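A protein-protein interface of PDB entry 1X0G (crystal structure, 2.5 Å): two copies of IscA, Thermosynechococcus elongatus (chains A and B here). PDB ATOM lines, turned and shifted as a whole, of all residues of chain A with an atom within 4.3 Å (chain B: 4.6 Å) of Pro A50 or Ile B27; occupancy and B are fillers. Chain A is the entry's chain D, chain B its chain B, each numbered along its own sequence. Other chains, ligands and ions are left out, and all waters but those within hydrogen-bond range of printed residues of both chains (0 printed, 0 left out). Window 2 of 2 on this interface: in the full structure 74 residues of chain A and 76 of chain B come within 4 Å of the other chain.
No position is printed for both chains. Of the 20 pairs that touch across the chains among the printed residues, none has its exchanged pair printed and touching as well.
The backbone NH (N) of Lys A51 is in hydrogen-bond range of the side-chain carboxylate (OD2) of Asp A54, at 2.8 Å.
Among the printed residues, merely in contact across the chains: Trp A62 with Ala B26, Lys A51 with Arg B29, Leu A46 with Ile B27, Ala A48 with Ile B27, Ala A65 with Arg B29, Val A47 with Ala B26, Pro A50 with Ile B27, Ala A45 with Leu B28, Ala A65 with Ile B27, Ala A48 with Ala B25, Thr A63 with Ile B27, Glu A49 with Ile B27, Val A47 with Ala B25 and Trp A62 with Leu B28.
Of the 13 printed residues of chain A, 11 touch a printed residue of chain B. Printed residues of chain A that touch a printed residue of chain B: Ala A45, Leu A46, Val A47, Ala A48, Glu A49, Pro A50, Lys A51, Asp A54, Trp A62, Thr A63 and Ala A65. Hydrophobic or aromatic side chains of chain A within 4 Å of the printed part of chain B: Leu A46, Val A47, Pro A50, Trp A62 and Ala A65. Among the printed residues, 20 pairs touch across the chains.
Of the printed residues of chain B, Glu A49 touches Ile B27 (3.9 Å). Of the printed residues of chain B, Pro A50 touches Ile B27. Printed residues of chain B within 4 Å of Lys A51: Arg B29. Of the printed residues of chain A, Ala B25 touches Val A47 and Ala A48. Printed residues of chain A within 4 Å of Ala B26: Val A47 and Trp A62. Of chain A, only Ala A45, Leu A46, Val A47, Ala A48, Glu A49, Pro A50, Thr A63 and Ala A65 come within 4 Å of Ile B27. Printed residues of chain A within 4 Å of Arg B29: Ala A45 (2.9 Å), Lys A51 (3.0 Å), Asp A54 (3.1 Å) and Ala A65 (3.2 Å). The nearest printed residue of chain B that does not touch Pro A50 is Arg B29 (4.8 Å). The nearest residue of chain A that does not touch Ile B27 is Trp A62 (4.2 Å). The nearest printed residue of chain A that does not touch Arg B29 is Val A47 (4.1 Å).
The backbone NH (N) of Ile B27 sits at hydrogen-bond distance from the backbone carbonyl oxygen (O) of Val A47. O of Thr A63 lies within hydrogen-bond range of N of Leu B28 (2.9 Å). O of Leu B28 lies within hydrogen-bond range of N of Ala A65 (2.7 Å). N of Arg B29 sits at hydrogen-bond distance from O of Ala A45 (2.9 Å). NE of Arg B29 lies within salt-bridge range of OD2 of Asp A54 (3.1 Å). The backbone carbonyl oxygen of Ala A45 sits close to the backbone carbonyl oxygen of Ile B27 (3.4 Å).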
ATOM      1  N   ALA A  45      23.105 -17.980   4.884  1.00  0.00           N
ATOM      2  CA  ALA A  45      22.659 -16.632   4.545  1.00  0.00           C
ATOM      3  C   ALA A  45      21.725 -16.831   3.375  1.00  0.00           C
ATOM      4  O   ALA A  45      21.830 -17.859   2.733  1.00  0.00           O
ATOM      5  CB  ALA A  45      23.814 -15.778   4.103  1.00  0.00           C
ATOM      6  N   LEU A  46      20.856 -15.859   3.097  1.00  0.00           N
ATOM      7  CA  LEU A  46      20.088 -15.781   1.868  1.00  0.00           C
ATOM      8  C   LEU A  46      20.676 -14.637   1.132  1.00  0.00           C
ATOM      9  O   LEU A  46      20.847 -13.603   1.743  1.00  0.00           O
ATOM     10  CB  LEU A  46      18.657 -15.384   2.157  1.00  0.00           C
ATOM     11  CG  LEU A  46      17.935 -16.491   2.900  1.00  0.00           C
ATOM     12  CD1 LEU A  46      16.496 -16.117   2.944  1.00  0.00           C
ATOM     13  CD2 LEU A  46      18.149 -17.897   2.270  1.00  0.00           C
ATOM     14  N   VAL A  47      20.956 -14.769  -0.156  1.00  0.00           N
ATOM     15  CA  VAL A  47      21.721 -13.743  -0.832  1.00  0.00           C
ATOM     16  C   VAL A  47      21.195 -13.612  -2.231  1.00  0.00           C
ATOM     17  O   VAL A  47      20.422 -14.442  -2.670  1.00  0.00           O
ATOM     18  CB  VAL A  47      23.252 -14.049  -0.851  1.00  0.00           C
ATOM     19  CG1 VAL A  47      23.774 -14.210   0.570  1.00  0.00           C
ATOM     20  CG2 VAL A  47      23.604 -15.259  -1.703  1.00  0.00           C
ATOM     21  N   ALA A  48      21.585 -12.584  -2.953  1.00  0.00           N
ATOM     22  CA  ALA A  48      20.849 -12.310  -4.190  1.00  0.00           C
ATOM     23  C   ALA A  48      21.432 -13.247  -5.200  1.00  0.00           C
ATOM     24  O   ALA A  48      20.712 -14.005  -5.865  1.00  0.00           O
ATOM     25  CB  ALA A  48      21.032 -10.867  -4.651  1.00  0.00           C
ATOM     26  N   GLU A  49      22.752 -13.148  -5.292  1.00  0.00           N
ATOM     27  CA  GLU A  49      23.551 -13.893  -6.216  1.00  0.00           C
ATOM     28  C   GLU A  49      24.530 -14.627  -5.313  1.00  0.00           C
ATOM     29  O   GLU A  49      24.710 -14.177  -4.181  1.00  0.00           O
ATOM     30  CB  GLU A  49      24.255 -12.931  -7.197  1.00  0.00           C
ATOM     31  CG  GLU A  49      23.499 -12.641  -8.575  1.00  0.00           C
ATOM     32  CD  GLU A  49      21.876 -12.701  -8.533  1.00  0.00           C
ATOM     33  OE1 GLU A  49      21.308 -13.735  -8.008  1.00  0.00           O
ATOM     34  OE2 GLU A  49      21.194 -11.731  -9.090  1.00  0.00           O
ATOM     35  N   PRO A  50      25.100 -15.775  -5.771  1.00  0.00           N
ATOM     36  CA  PRO A  50      26.298 -16.472  -5.262  1.00  0.00           C
ATOM     37  C   PRO A  50      27.567 -15.734  -5.645  1.00  0.00           C
ATOM     38  O   PRO A  50      27.503 -14.855  -6.523  1.00  0.00           O
ATOM     39  CB  PRO A  50      26.303 -17.747  -6.085  1.00  0.00           C
ATOM     40  CG  PRO A  50      25.697 -17.305  -7.338  1.00  0.00           C
ATOM     41  CD  PRO A  50      24.531 -16.548  -6.873  1.00  0.00           C
ATOM     42  N   LYS A  51      28.683 -16.087  -5.006  1.00  0.00           N
ATOM     43  CA  LYS A  51      29.988 -15.609  -5.425  1.00  0.00           C
ATOM     44  C   LYS A  51      30.360 -16.362  -6.718  1.00  0.00           C
ATOM     45  O   LYS A  51      29.973 -17.528  -6.938  1.00  0.00           O
ATOM     46  CB  LYS A  51      31.081 -15.772  -4.339  1.00  0.00           C
ATOM     47  CG  LYS A  51      30.742 -15.284  -2.905  1.00  0.00           C
ATOM     48  CD  LYS A  51      31.923 -14.570  -2.205  1.00  0.00           C
ATOM     49  CE  LYS A  51      32.561 -13.550  -3.249  1.00  0.00           C
ATOM     50  NZ  LYS A  51      33.461 -12.451  -2.712  1.00  0.00           N
ATOM     51  N   PRO A  52      31.094 -15.702  -7.609  1.00  0.00           N
ATOM     52  CA  PRO A  52      31.234 -16.421  -8.866  1.00  0.00           C
ATOM     53  C   PRO A  52      32.030 -17.756  -8.726  1.00  0.00           C
ATOM     54  O   PRO A  52      31.986 -18.602  -9.620  1.00  0.00           O
ATOM     55  CB  PRO A  52      31.971 -15.415  -9.773  1.00  0.00           C
ATOM     56  CG  PRO A  52      32.686 -14.485  -8.825  1.00  0.00           C
ATOM     57  CD  PRO A  52      31.828 -14.427  -7.589  1.00  0.00           C
ATOM     58  N   ASP A  54      31.528 -20.042  -6.285  1.00  0.00           N
ATOM     59  CA  ASP A  54      30.861 -21.095  -5.531  1.00  0.00           C
ATOM     60  C   ASP A  54      30.360 -22.206  -6.406  1.00  0.00           C
ATOM     61  O   ASP A  54      30.196 -22.087  -7.612  1.00  0.00           O
ATOM     62  CB  ASP A  54      29.679 -20.577  -4.740  1.00  0.00           C
ATOM     63  CG  ASP A  54      30.046 -19.464  -3.814  1.00  0.00           C
ATOM     64  OD1 ASP A  54      31.136 -19.509  -3.155  1.00  0.00           O
ATOM     65  OD2 ASP A  54      29.214 -18.537  -3.748  1.00  0.00           O
ATOM     66  N   LEU A  56      27.263 -24.463  -7.156  1.00  0.00           N
ATOM     67  CA  LEU A  56      25.793 -24.423  -7.117  1.00  0.00           C
ATOM     68  C   LEU A  56      25.118 -25.797  -7.059  1.00  0.00           C
ATOM     69  O   LEU A  56      25.496 -26.708  -7.783  1.00  0.00           O
ATOM     70  CB  LEU A  56      25.293 -23.673  -8.355  1.00  0.00           C
ATOM     71  CG  LEU A  56      25.807 -22.234  -8.294  1.00  0.00           C
ATOM     72  CD1 LEU A  56      25.366 -21.481  -9.523  1.00  0.00           C
ATOM     73  CD2 LEU A  56      25.292 -21.570  -7.064  1.00  0.00           C
ATOM     74  N   TRP A  62      15.253 -25.172  -4.031  1.00  0.00           N
ATOM     75  CA  TRP A  62      16.088 -24.106  -3.464  1.00  0.00           C
ATOM     76  C   TRP A  62      17.401 -24.123  -4.138  1.00  0.00           C
ATOM     77  O   TRP A  62      18.050 -25.166  -4.196  1.00  0.00           O
ATOM     78  CB  TRP A  62      16.335 -24.263  -1.924  1.00  0.00           C
ATOM     79  CG  TRP A  62      15.369 -23.397  -1.191  1.00  0.00           C
ATOM     80  CD1 TRP A  62      14.121 -23.737  -0.792  1.00  0.00           C
ATOM     81  CD2 TRP A  62      15.516 -22.011  -0.894  1.00  0.00           C
ATOM     82  NE1 TRP A  62      13.454 -22.643  -0.246  1.00  0.00           N
ATOM     83  CE2 TRP A  62      14.282 -21.568  -0.308  1.00  0.00           C
ATOM     84  CE3 TRP A  62      16.545 -21.090  -1.090  1.00  0.00           C
ATOM     85  CZ2 TRP A  62      14.074 -20.274   0.117  1.00  0.00           C
ATOM     86  CZ3 TRP A  62      16.340 -19.796  -0.670  1.00  0.00           C
ATOM     87  CH2 TRP A  62      15.108 -19.395  -0.065  1.00  0.00           C
ATOM     88  N   THR A  63      17.804 -22.968  -4.635  1.00  0.00           N
ATOM     89  CA  THR A  63      19.206 -22.801  -4.965  1.00  0.00           C
ATOM     90  C   THR A  63      20.114 -22.686  -3.688  1.00  0.00           C
ATOM     91  O   THR A  63      19.828 -21.964  -2.731  1.00  0.00           O
ATOM     92  CB  THR A  63      19.423 -21.608  -5.883  1.00  0.00           C
ATOM     93  OG1 THR A  63      18.545 -21.703  -7.018  1.00  0.00           O
ATOM     94  CG2 THR A  63      20.866 -21.594  -6.384  1.00  0.00           C
ATOM     95  N   ALA A  65      24.158 -22.024  -2.737  1.00  0.00           N
ATOM     96  CA  ALA A  65      25.492 -21.810  -3.212  1.00  0.00           C
ATOM     97  C   ALA A  65      26.433 -22.253  -2.084  1.00  0.00           C
ATOM     98  O   ALA A  65      26.181 -22.005  -0.919  1.00  0.00           O
ATOM     99  CB  ALA A  65      25.710 -20.400  -3.647  1.00  0.00           C
ATOM    100  N   ALA B  25      15.265 -12.290  -5.729  1.00  0.00           N
ATOM    101  CA  ALA B  25      16.006 -13.598  -5.799  1.00  0.00           C
ATOM    102  C   ALA B  25      16.580 -13.923  -4.423  1.00  0.00           C
ATOM    103  O   ALA B  25      16.911 -12.984  -3.706  1.00  0.00           O
ATOM    104  CB  ALA B  25      17.156 -13.534  -6.868  1.00  0.00           C
ATOM    105  N   ALA B  26      16.675 -15.198  -4.018  1.00  0.00           N
ATOM    106  CA  ALA B  26      17.255 -15.530  -2.696  1.00  0.00           C
ATOM    107  C   ALA B  26      17.821 -16.905  -2.696  1.00  0.00           C
ATOM    108  O   ALA B  26      17.083 -17.870  -2.678  1.00  0.00           O
ATOM    109  CB  ALA B  26      16.259 -15.404  -1.584  1.00  0.00           C
ATOM    110  N   ILE B  27      19.144 -16.996  -2.679  1.00  0.00           N
ATOM    111  CA  ILE B  27      19.885 -18.234  -2.645  1.00  0.00           C
ATOM    112  C   ILE B  27      20.359 -18.550  -1.234  1.00  0.00           C
ATOM    113  O   ILE B  27      20.775 -17.692  -0.474  1.00  0.00           O
ATOM    114  CB  ILE B  27      21.057 -18.013  -3.509  1.00  0.00           C
ATOM    115  CG1 ILE B  27      20.545 -17.951  -4.922  1.00  0.00           C
ATOM    116  CG2 ILE B  27      22.206 -19.042  -3.257  1.00  0.00           C
ATOM    117  CD1 ILE B  27      21.398 -17.061  -5.725  1.00  0.00           C
ATOM    118  N   LEU B  28      20.304 -19.811  -0.880  1.00  0.00           N
ATOM    119  CA  LEU B  28      20.840 -20.242   0.350  1.00  0.00           C
ATOM    120  C   LEU B  28      22.305 -20.404   0.121  1.00  0.00           C
ATOM    121  O   LEU B  28      22.683 -21.199  -0.687  1.00  0.00           O
ATOM    122  CB  LEU B  28      20.265 -21.578   0.673  1.00  0.00           C
ATOM    123  CG  LEU B  28      20.845 -22.070   1.965  1.00  0.00           C
ATOM    124  CD1 LEU B  28      20.646 -21.073   3.124  1.00  0.00           C
ATOM    125  CD2 LEU B  28      20.116 -23.366   2.209  1.00  0.00           C
ATOM    126  N   ARG B  29      23.121 -19.616   0.811  1.00  0.00           N
ATOM    127  CA  ARG B  29      24.583 -19.728   0.749  1.00  0.00           C
ATOM    128  C   ARG B  29      25.169 -20.275   2.057  1.00  0.00           C
ATOM    129  O   ARG B  29      24.921 -19.809   3.160  1.00  0.00           O
ATOM    130  CB  ARG B  29      25.203 -18.410   0.369  1.00  0.00           C
ATOM    131  CG  ARG B  29      26.658 -18.465   0.113  1.00  0.00           C
ATOM    132  CD  ARG B  29      27.101 -17.189  -0.568  1.00  0.00           C
ATOM    133  NE  ARG B  29      28.457 -17.256  -1.066  1.00  0.00           N
ATOM    134  CZ  ARG B  29      29.547 -17.327  -0.285  1.00  0.00           C
ATOM    135  NH1 ARG B  29      29.437 -17.313   1.051  1.00  0.00           N
ATOM    136  NH2 ARG B  29      30.765 -17.392  -0.838  1.00  0.00           N
